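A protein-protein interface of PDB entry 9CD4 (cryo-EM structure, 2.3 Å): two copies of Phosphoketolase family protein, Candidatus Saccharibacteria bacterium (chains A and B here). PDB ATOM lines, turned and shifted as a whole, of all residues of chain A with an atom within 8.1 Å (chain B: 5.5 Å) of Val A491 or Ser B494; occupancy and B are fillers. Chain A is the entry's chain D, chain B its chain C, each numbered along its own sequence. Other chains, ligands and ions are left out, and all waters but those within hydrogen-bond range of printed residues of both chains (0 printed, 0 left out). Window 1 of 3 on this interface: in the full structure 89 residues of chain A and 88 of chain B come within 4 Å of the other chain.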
ATOM      1  N   TYR A 161      21.327  25.704  -4.061  1.00  0.00           N
ATOM      2  CA  TYR A 161      21.059  24.285  -3.830  1.00  0.00           C
ATOM      3  C   TYR A 161      21.188  23.462  -5.105  1.00  0.00           C
ATOM      4  O   TYR A 161      20.417  22.525  -5.323  1.00  0.00           O
ATOM      5  CB  TYR A 161      19.676  24.094  -3.216  1.00  0.00           C
ATOM      6  CG  TYR A 161      19.339  25.052  -2.094  1.00  0.00           C
ATOM      7  CD1 TYR A 161      20.262  25.348  -1.098  1.00  0.00           C
ATOM      8  CD2 TYR A 161      18.088  25.651  -2.026  1.00  0.00           C
ATOM      9  CE1 TYR A 161      19.950  26.223  -0.074  1.00  0.00           C
ATOM     10  CE2 TYR A 161      17.768  26.521  -1.006  1.00  0.00           C
ATOM     11  CZ  TYR A 161      18.701  26.805  -0.033  1.00  0.00           C
ATOM     12  OH  TYR A 161      18.381  27.674   0.984  1.00  0.00           O
ATOM     13  N   SER A 191      26.141  27.663   0.641  1.00  0.00           N
ATOM     14  CA  SER A 191      25.817  26.287   0.280  1.00  0.00           C
ATOM     15  C   SER A 191      26.699  25.788  -0.859  1.00  0.00           C
ATOM     16  O   SER A 191      27.197  24.658  -0.817  1.00  0.00           O
ATOM     17  CB  SER A 191      24.341  26.178  -0.096  1.00  0.00           C
ATOM     18  OG  SER A 191      23.517  26.729   0.915  1.00  0.00           O
ATOM     19  N   LEU A 461      29.963  18.077   8.114  1.00  0.00           N
ATOM     20  CA  LEU A 461      29.344  18.972   9.083  1.00  0.00           C
ATOM     21  C   LEU A 461      28.382  19.971   8.453  1.00  0.00           C
ATOM     22  O   LEU A 461      27.648  20.644   9.186  1.00  0.00           O
ATOM     23  CB  LEU A 461      30.425  19.714   9.872  1.00  0.00           C
ATOM     24  CG  LEU A 461      30.350  19.541  11.391  1.00  0.00           C
ATOM     25  CD1 LEU A 461      31.707  19.771  12.026  1.00  0.00           C
ATOM     26  CD2 LEU A 461      29.317  20.480  11.994  1.00  0.00           C
ATOM     27  N   SER A 462      28.356  20.083   7.128  1.00  0.00           N
ATOM     28  CA  SER A 462      27.436  20.990   6.452  1.00  0.00           C
ATOM     29  C   SER A 462      26.070  20.323   6.348  1.00  0.00           C
ATOM     30  O   SER A 462      25.903  19.345   5.613  1.00  0.00           O
ATOM     31  CB  SER A 462      27.973  21.364   5.074  1.00  0.00           C
ATOM     32  OG  SER A 462      27.090  22.245   4.405  1.00  0.00           O
ATOM     33  N   GLU A 463      25.090  20.849   7.088  1.00  0.00           N
ATOM     34  CA  GLU A 463      23.740  20.299   7.033  1.00  0.00           C
ATOM     35  C   GLU A 463      23.073  20.575   5.692  1.00  0.00           C
ATOM     36  O   GLU A 463      22.230  19.786   5.245  1.00  0.00           O
ATOM     37  CB  GLU A 463      22.893  20.869   8.170  1.00  0.00           C
ATOM     38  CG  GLU A 463      23.279  20.364   9.552  1.00  0.00           C
ATOM     39  CD  GLU A 463      24.368  21.198  10.200  1.00  0.00           C
ATOM     40  OE1 GLU A 463      24.885  22.125   9.542  1.00  0.00           O
ATOM     41  OE2 GLU A 463      24.707  20.926  11.370  1.00  0.00           O
ATOM     42  N   ASN A 464      23.427  21.691   5.047  1.00  0.00           N
ATOM     43  CA  ASN A 464      22.870  22.010   3.736  1.00  0.00           C
ATOM     44  C   ASN A 464      23.273  20.969   2.701  1.00  0.00           C
ATOM     45  O   ASN A 464      22.456  20.566   1.864  1.00  0.00           O
ATOM     46  CB  ASN A 464      23.321  23.404   3.302  1.00  0.00           C
ATOM     47  CG  ASN A 464      22.855  24.492   4.250  1.00  0.00           C
ATOM     48  OD1 ASN A 464      21.666  24.614   4.539  1.00  0.00           O
ATOM     49  ND2 ASN A 464      23.796  25.290   4.740  1.00  0.00           N
ATOM     50  N   GLN A 467      21.180  17.834   3.315  1.00  0.00           N
ATOM     51  CA  GLN A 467      19.817  17.987   2.814  1.00  0.00           C
ATOM     52  C   GLN A 467      19.779  17.931   1.291  1.00  0.00           C
ATOM     53  O   GLN A 467      18.873  17.319   0.709  1.00  0.00           O
ATOM     54  CB  GLN A 467      19.214  19.294   3.326  1.00  0.00           C
ATOM     55  CG  GLN A 467      17.857  19.623   2.735  1.00  0.00           C
ATOM     56  CD  GLN A 467      16.755  18.737   3.270  1.00  0.00           C
ATOM     57  OE1 GLN A 467      16.838  18.229   4.387  1.00  0.00           O
ATOM     58  NE2 GLN A 467      15.712  18.547   2.473  1.00  0.00           N
ATOM     59  N   SER A 484      20.054  13.880  12.864  1.00  0.00           N
ATOM     60  CA  SER A 484      20.748  15.068  13.357  1.00  0.00           C
ATOM     61  C   SER A 484      20.322  15.344  14.797  1.00  0.00           C
ATOM     62  O   SER A 484      19.470  14.651  15.367  1.00  0.00           O
ATOM     63  CB  SER A 484      20.472  16.287  12.470  1.00  0.00           C
ATOM     64  OG  SER A 484      21.341  17.360  12.789  1.00  0.00           O
ATOM     65  N   GLU A 486      18.426  17.908  17.459  1.00  0.00           N
ATOM     66  CA  GLU A 486      17.208  18.702  17.346  1.00  0.00           C
ATOM     67  C   GLU A 486      17.512  20.193  17.254  1.00  0.00           C
ATOM     68  O   GLU A 486      16.778  20.935  16.591  1.00  0.00           O
ATOM     69  CB  GLU A 486      16.288  18.415  18.531  1.00  0.00           C
ATOM     70  CG  GLU A 486      14.924  19.066  18.429  1.00  0.00           C
ATOM     71  CD  GLU A 486      14.074  18.827  19.657  1.00  0.00           C
ATOM     72  OE1 GLU A 486      14.455  19.302  20.747  1.00  0.00           O
ATOM     73  OE2 GLU A 486      13.025  18.163  19.532  1.00  0.00           O
ATOM     74  N   ALA A 487      18.591  20.647  17.894  1.00  0.00           N
ATOM     75  CA  ALA A 487      18.878  22.075  17.972  1.00  0.00           C
ATOM     76  C   ALA A 487      19.384  22.652  16.656  1.00  0.00           C
ATOM     77  O   ALA A 487      19.072  23.803  16.331  1.00  0.00           O
ATOM     78  CB  ALA A 487      19.897  22.346  19.079  1.00  0.00           C
ATOM     79  N   PHE A 488      20.160  21.886  15.891  1.00  0.00           N
ATOM     80  CA  PHE A 488      20.770  22.376  14.663  1.00  0.00           C
ATOM     81  C   PHE A 488      19.965  22.023  13.420  1.00  0.00           C
ATOM     82  O   PHE A 488      20.431  22.262  12.301  1.00  0.00           O
ATOM     83  CB  PHE A 488      22.198  21.841  14.545  1.00  0.00           C
ATOM     84  CG  PHE A 488      23.036  22.100  15.762  1.00  0.00           C
ATOM     85  CD1 PHE A 488      23.183  23.386  16.253  1.00  0.00           C
ATOM     86  CD2 PHE A 488      23.662  21.059  16.424  1.00  0.00           C
ATOM     87  CE1 PHE A 488      23.947  23.632  17.378  1.00  0.00           C
ATOM     88  CE2 PHE A 488      24.427  21.298  17.551  1.00  0.00           C
ATOM     89  CZ  PHE A 488      24.571  22.585  18.026  1.00  0.00           C
ATOM     90  N   ALA A 489      18.774  21.442  13.592  1.00  0.00           N
ATOM     91  CA  ALA A 489      17.888  21.207  12.451  1.00  0.00           C
ATOM     92  C   ALA A 489      17.431  22.487  11.748  1.00  0.00           C
ATOM     93  O   ALA A 489      17.446  22.508  10.504  1.00  0.00           O
ATOM     94  CB  ALA A 489      16.699  20.348  12.890  1.00  0.00           C
ATOM     95  N   PRO A 490      17.010  23.570  12.442  1.00  0.00           N
ATOM     96  CA  PRO A 490      16.471  24.734  11.705  1.00  0.00           C
ATOM     97  C   PRO A 490      17.422  25.382  10.706  1.00  0.00           C
ATOM     98  O   PRO A 490      16.971  26.194   9.885  1.00  0.00           O
ATOM     99  CB  PRO A 490      16.104  25.713  12.828  1.00  0.00           C
ATOM    100  CG  PRO A 490      15.796  24.860  13.965  1.00  0.00           C
ATOM    101  CD  PRO A 490      16.781  23.742  13.893  1.00  0.00           C
ATOM    102  N   VAL A 491      18.707  25.024  10.729  1.00  0.00           N
ATOM    103  CA  VAL A 491      19.694  25.491   9.760  1.00  0.00           C
ATOM    104  C   VAL A 491      19.240  25.130   8.350  1.00  0.00           C
ATOM    105  O   VAL A 491      19.484  25.879   7.396  1.00  0.00           O
ATOM    106  CB  VAL A 491      21.082  24.897  10.073  1.00  0.00           C
ATOM    107  CG1 VAL A 491      22.123  25.360   9.064  1.00  0.00           C
ATOM    108  CG2 VAL A 491      21.508  25.270  11.482  1.00  0.00           C
ATOM    109  N   ILE A 492      18.543  24.003   8.207  1.00  0.00           N
ATOM    110  CA  ILE A 492      18.051  23.595   6.896  1.00  0.00           C
ATOM    111  C   ILE A 492      16.532  23.709   6.827  1.00  0.00           C
ATOM    112  O   ILE A 492      15.878  22.953   6.099  1.00  0.00           O
ATOM    113  CB  ILE A 492      18.544  22.177   6.531  1.00  0.00           C
ATOM    114  CG1 ILE A 492      18.410  21.187   7.698  1.00  0.00           C
ATOM    115  CG2 ILE A 492      19.982  22.225   6.062  1.00  0.00           C
ATOM    116  CD1 ILE A 492      17.050  20.537   7.874  1.00  0.00           C
ATOM    117  N   SER A 493      15.960  24.658   7.577  1.00  0.00           N
ATOM    118  CA  SER A 493      14.513  24.863   7.539  1.00  0.00           C
ATOM    119  C   SER A 493      14.043  25.307   6.158  1.00  0.00           C
ATOM    120  O   SER A 493      13.293  24.591   5.483  1.00  0.00           O
ATOM    121  CB  SER A 493      14.095  25.888   8.594  1.00  0.00           C
ATOM    122  OG  SER A 493      13.906  25.280   9.856  1.00  0.00           O
ATOM    123  N   SER A 494      14.501  26.485   5.716  1.00  0.00           N
ATOM    124  CA  SER A 494      13.908  27.150   4.555  1.00  0.00           C
ATOM    125  C   SER A 494      14.040  26.312   3.290  1.00  0.00           C
ATOM    126  O   SER A 494      13.077  26.186   2.522  1.00  0.00           O
ATOM    127  CB  SER A 494      14.556  28.518   4.353  1.00  0.00           C
ATOM    128  OG  SER A 494      15.840  28.388   3.766  1.00  0.00           O
ATOM    129  N   MET A 495      15.216  25.715   3.073  1.00  0.00           N
ATOM    130  CA  MET A 495      15.416  24.861   1.905  1.00  0.00           C
ATOM    131  C   MET A 495      14.434  23.698   1.911  1.00  0.00           C
ATOM    132  O   MET A 495      13.862  23.356   0.867  1.00  0.00           O
ATOM    133  CB  MET A 495      16.860  24.355   1.867  1.00  0.00           C
ATOM    134  CG  MET A 495      17.035  22.987   1.228  1.00  0.00           C
ATOM    135  SD  MET A 495      18.754  22.555   0.890  1.00  0.00           S
ATOM    136  CE  MET A 495      19.601  23.445   2.189  1.00  0.00           C
ATOM    137  N   MET A 496      14.192  23.115   3.091  1.00  0.00           N
ATOM    138  CA  MET A 496      13.190  22.060   3.216  1.00  0.00           C
ATOM    139  C   MET A 496      11.829  22.545   2.740  1.00  0.00           C
ATOM    140  O   MET A 496      11.130  21.828   2.011  1.00  0.00           O
ATOM    141  CB  MET A 496      13.114  21.580   4.665  1.00  0.00           C
ATOM    142  CG  MET A 496      12.094  20.478   4.909  1.00  0.00           C
ATOM    143  SD  MET A 496      10.527  21.066   5.587  1.00  0.00           S
ATOM    144  CE  MET A 496      11.086  22.359   6.692  1.00  0.00           C
ATOM    145  N   ASN A 538      16.643  24.044  21.058  1.00  0.00           N
ATOM    146  CA  ASN A 538      15.871  24.811  20.080  1.00  0.00           C
ATOM    147  C   ASN A 538      14.901  23.882  19.367  1.00  0.00           C
ATOM    148  O   ASN A 538      15.207  23.339  18.298  1.00  0.00           O
ATOM    149  CB  ASN A 538      16.782  25.514  19.074  1.00  0.00           C
ATOM    150  CG  ASN A 538      16.076  26.625  18.327  1.00  0.00           C
ATOM    151  OD1 ASN A 538      15.072  27.162  18.794  1.00  0.00           O
ATOM    152  ND2 ASN A 538      16.599  26.978  17.160  1.00  0.00           N
ATOM    153  N   SER A 540      12.322  24.123  17.295  1.00  0.00           N
ATOM    154  CA  SER A 540      11.544  24.927  16.361  1.00  0.00           C
ATOM    155  C   SER A 540      11.417  24.314  14.973  1.00  0.00           C
ATOM    156  O   SER A 540      10.655  24.839  14.154  1.00  0.00           O
ATOM    157  CB  SER A 540      12.151  26.333  16.239  1.00  0.00           C
ATOM    158  OG  SER A 540      13.428  26.293  15.629  1.00  0.00           O
ATOM    159  N   PHE A 541      12.139  23.227  14.682  1.00  0.00           N
ATOM    160  CA  PHE A 541      12.069  22.623  13.354  1.00  0.00           C
ATOM    161  C   PHE A 541      10.719  21.958  13.110  1.00  0.00           C
ATOM    162  O   PHE A 541      10.199  21.990  11.986  1.00  0.00           O
ATOM    163  CB  PHE A 541      13.204  21.617  13.179  1.00  0.00           C
ATOM    164  CG  PHE A 541      13.302  21.050  11.794  1.00  0.00           C
ATOM    165  CD1 PHE A 541      13.861  21.789  10.766  1.00  0.00           C
ATOM    166  CD2 PHE A 541      12.844  19.771  11.520  1.00  0.00           C
ATOM    167  CE1 PHE A 541      13.953  21.271   9.490  1.00  0.00           C
ATOM    168  CE2 PHE A 541      12.935  19.244  10.245  1.00  0.00           C
ATOM    169  CZ  PHE A 541      13.491  19.996   9.228  1.00  0.00           C
ATOM    170  N   GLU B 158      26.406  26.983  18.429  1.00  0.00           N
ATOM    171  CA  GLU B 158      26.175  26.577  17.050  1.00  0.00           C
ATOM    172  C   GLU B 158      27.401  26.932  16.220  1.00  0.00           C
ATOM    173  O   GLU B 158      27.800  28.100  16.164  1.00  0.00           O
ATOM    174  CB  GLU B 158      24.926  27.258  16.497  1.00  0.00           C
ATOM    175  CG  GLU B 158      24.435  26.686  15.177  1.00  0.00           C
ATOM    176  CD  GLU B 158      23.020  27.119  14.846  1.00  0.00           C
ATOM    177  OE1 GLU B 158      22.111  26.862  15.663  1.00  0.00           O
ATOM    178  OE2 GLU B 158      22.815  27.718  13.771  1.00  0.00           O
ATOM    179  N   TYR B 161      29.483  31.106  12.051  1.00  0.00           N
ATOM    180  CA  TYR B 161      29.178  32.496  12.411  1.00  0.00           C
ATOM    181  C   TYR B 161      30.306  33.135  13.218  1.00  0.00           C
ATOM    182  O   TYR B 161      30.057  33.944  14.113  1.00  0.00           O
ATOM    183  CB  TYR B 161      27.854  32.620  13.179  1.00  0.00           C
ATOM    184  CG  TYR B 161      26.789  31.592  12.851  1.00  0.00           C
ATOM    185  CD1 TYR B 161      26.432  31.310  11.536  1.00  0.00           C
ATOM    186  CD2 TYR B 161      26.129  30.910  13.866  1.00  0.00           C
ATOM    187  CE1 TYR B 161      25.460  30.373  11.245  1.00  0.00           C
ATOM    188  CE2 TYR B 161      25.155  29.975  13.584  1.00  0.00           C
ATOM    189  CZ  TYR B 161      24.823  29.710  12.273  1.00  0.00           C
ATOM    190  OH  TYR B 161      23.853  28.778  11.987  1.00  0.00           O
ATOM    191  N   PRO B 490      14.141  33.273   6.119  1.00  0.00           N
ATOM    192  CA  PRO B 490      14.411  32.129   7.011  1.00  0.00           C
ATOM    193  C   PRO B 490      15.759  31.445   6.814  1.00  0.00           C
ATOM    194  O   PRO B 490      16.141  30.593   7.624  1.00  0.00           O
ATOM    195  CB  PRO B 490      13.262  31.162   6.696  1.00  0.00           C
ATOM    196  CG  PRO B 490      12.181  32.025   6.202  1.00  0.00           C
ATOM    197  CD  PRO B 490      12.875  33.059   5.386  1.00  0.00           C
ATOM    198  N   VAL B 491      16.488  31.819   5.757  1.00  0.00           N
ATOM    199  CA  VAL B 491      17.849  31.327   5.560  1.00  0.00           C
ATOM    200  C   VAL B 491      18.730  31.701   6.748  1.00  0.00           C
ATOM    201  O   VAL B 491      19.614  30.935   7.151  1.00  0.00           O
ATOM    202  CB  VAL B 491      18.418  31.867   4.234  1.00  0.00           C
ATOM    203  CG1 VAL B 491      19.829  31.351   3.992  1.00  0.00           C
ATOM    204  CG2 VAL B 491      17.508  31.492   3.078  1.00  0.00           C
ATOM    205  N   ILE B 492      18.486  32.867   7.348  1.00  0.00           N
ATOM    206  CA  ILE B 492      19.236  33.269   8.534  1.00  0.00           C
ATOM    207  C   ILE B 492      18.358  33.143   9.772  1.00  0.00           C
ATOM    208  O   ILE B 492      18.551  33.862  10.759  1.00  0.00           O
ATOM    209  CB  ILE B 492      19.822  34.691   8.377  1.00  0.00           C
ATOM    210  CG1 ILE B 492      18.815  35.695   7.790  1.00  0.00           C
ATOM    211  CG2 ILE B 492      21.065  34.651   7.524  1.00  0.00           C
ATOM    212  CD1 ILE B 492      17.816  36.298   8.764  1.00  0.00           C
ATOM    213  N   SER B 493      17.389  32.226   9.723  1.00  0.00           N
ATOM    214  CA  SER B 493      16.461  32.049  10.835  1.00  0.00           C
ATOM    215  C   SER B 493      17.180  31.586  12.100  1.00  0.00           C
ATOM    216  O   SER B 493      17.236  32.316  13.098  1.00  0.00           O
ATOM    217  CB  SER B 493      15.370  31.052  10.444  1.00  0.00           C
ATOM    218  OG  SER B 493      14.209  31.229  11.231  1.00  0.00           O
ATOM    219  N   SER B 494      17.769  30.386  12.056  1.00  0.00           N
ATOM    220  CA  SER B 494      18.270  29.735  13.264  1.00  0.00           C
ATOM    221  C   SER B 494      19.374  30.545  13.929  1.00  0.00           C
ATOM    222  O   SER B 494      19.393  30.686  15.159  1.00  0.00           O
ATOM    223  CB  SER B 494      18.774  28.332  12.930  1.00  0.00           C
ATOM    224  OG  SER B 494      20.033  28.389  12.282  1.00  0.00           O
ATOM    225  N   MET B 495      20.288  31.104  13.127  1.00  0.00           N
ATOM    226  CA  MET B 495      21.360  31.933  13.670  1.00  0.00           C
ATOM    227  C   MET B 495      20.795  33.111  14.453  1.00  0.00           C
ATOM    228  O   MET B 495      21.298  33.446  15.534  1.00  0.00           O
ATOM    229  CB  MET B 495      22.268  32.418  12.539  1.00  0.00           C
ATOM    230  CG  MET B 495      22.951  33.750  12.803  1.00  0.00           C
ATOM    231  SD  MET B 495      24.281  34.130  11.646  1.00  0.00           S
ATOM    232  CE  MET B 495      23.693  33.319  10.164  1.00  0.00           C
ATOM    233  N   MET B 496      19.709  33.709  13.948  1.00  0.00           N
ATOM    234  CA  MET B 496      19.058  34.802  14.662  1.00  0.00           C
ATOM    235  C   MET B 496      18.609  34.356  16.046  1.00  0.00           C
ATOM    236  O   MET B 496      18.799  35.083  17.030  1.00  0.00           O
ATOM    237  CB  MET B 496      17.872  35.322  13.848  1.00  0.00           C
ATOM    238  CG  MET B 496      16.968  36.282  14.598  1.00  0.00           C
ATOM    239  SD  MET B 496      15.447  35.502  15.170  1.00  0.00           S
ATOM    240  CE  MET B 496      14.920  34.639  13.693  1.00  0.00           C
ATOM    241  N   ASP B 497      18.065  33.134  16.143  1.00  0.00           N
ATOM    242  CA  ASP B 497      17.656  32.595  17.437  1.00  0.00           C
ATOM    243  C   ASP B 497      18.825  32.557  18.411  1.00  0.00           C
ATOM    244  O   ASP B 497      18.663  32.884  19.594  1.00  0.00           O
ATOM    245  CB  ASP B 497      17.064  31.196  17.262  1.00  0.00           C
ATOM    246  CG  ASP B 497      15.583  31.224  16.947  1.00  0.00           C
ATOM    247  OD1 ASP B 497      14.813  31.791  17.750  1.00  0.00           O
ATOM    248  OD2 ASP B 497      15.189  30.675  15.898  1.00  0.00           O
ATOM    249  N   GLN B 498      20.019  32.211  17.912  1.00  0.00           N
ATOM    250  CA  GLN B 498      21.212  32.208  18.754  1.00  0.00           C
ATOM    251  C   GLN B 498      21.430  33.578  19.380  1.00  0.00           C
ATOM    252  O   GLN B 498      21.632  33.692  20.598  1.00  0.00           O
ATOM    253  CB  GLN B 498      22.432  31.792  17.932  1.00  0.00           C
ATOM    254  CG  GLN B 498      22.484  30.314  17.589  1.00  0.00           C
ATOM    255  CD  GLN B 498      23.052  29.473  18.713  1.00  0.00           C
ATOM    256  OE1 GLN B 498      24.260  29.469  18.952  1.00  0.00           O
ATOM    257  NE2 GLN B 498      22.182  28.750  19.410  1.00  0.00           N
ATOM    258  N   GLU B 544       8.998  32.645  13.454  1.00  0.00           N
ATOM    259  CA  GLU B 544      10.195  32.327  14.223  1.00  0.00           C
ATOM    260  C   GLU B 544      10.608  33.483  15.123  1.00  0.00           C
ATOM    261  O   GLU B 544      11.139  33.254  16.216  1.00  0.00           O
ATOM    262  CB  GLU B 544      11.343  31.954  13.286  1.00  0.00           C
ATOM    263  CG  GLU B 544      12.506  31.263  13.981  1.00  0.00           C
ATOM    264  CD  GLU B 544      12.430  29.750  13.898  1.00  0.00           C
ATOM    265  OE1 GLU B 544      11.420  29.176  14.355  1.00  0.00           O
ATOM    266  OE2 GLU B 544      13.384  29.134  13.377  1.00  0.00           O
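The side-chain hydroxyl (OG) of Ser B493 sits at hydrogen-bond distance from the side-chain carboxylate (OE2) of Glu B544, at 3.1 Å. The side-chain hydroxyl of Ser B494 sits at hydrogen-bond distance from the side-chain carboxylate of Glu B158, 3.2 Å away. O of Pro A490 lies close to OG of Ser A493. N of Glu B158 lies within hydrogen-bond range of OE1 of Gln B498.
Pro A490 touches Ser B494, and with the chains exchanged Ser A494 touches Pro B490. Val A491 touches Ser B494, and with the chains exchanged Ser A494 touches Val B491. Of the 7 pairs that touch across the chains among the printed residues, 4 have their exchanged pair printed and touching as well.
Printed residues of chain B within 4 Å of Phe A488: Glu B158. Val A491 touches just these residues of chain B: Glu B158 and Ser B494. Of the printed residues of chain B, Ser A494 touches Pro B490 and Val B491. Printed residues of chain A within 4 Å of Glu B158: Phe A488 (3.7 Å) and Val A491 (3.6 Å). Of the printed residues of chain A, Pro B490 touches Ser A494 (3.8 Å). No residue of chain A comes within 4 Å of Ser B493. Ser B494 touches two residues of chain A. The nearest residue of chain A that does not touch Ser B494 is Asn A538 (4.9 Å).
CD1 of Phe A488 touches OE1 of Glu B158, at 3.7 Å. Pro A490 touches Ser B494 (CB to CB, 3.7 Å). CG2 of Val A491 touches OE2 of Glu B158, 3.6 Å away. Ser B494 touches Val A491 (OG to CG2, 3.5 Å). Ser A494 touches Pro B490. CG2 of Val B491 touches OG of Ser A494 (3.6 Å). Ser A540 touches Glu B544.
Printed residues of chain B that touch a printed residue of chain A: Glu B158, Pro B490, Val B491, Ser B494 and Glu B544. Hydrophobic or aromatic side chains of chain B that line the printed part of chain A: Pro B490 and Val B491. Along chain A the printed residues that touch a printed residue of chain B span positions 488 to 540. Among the printed residues, 7 pairs touch across the chains. Among the printed residues, no Asp or Glu carboxylate lies within 4 Å of a Lys or Arg side-chain nitrogen of the other chain.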
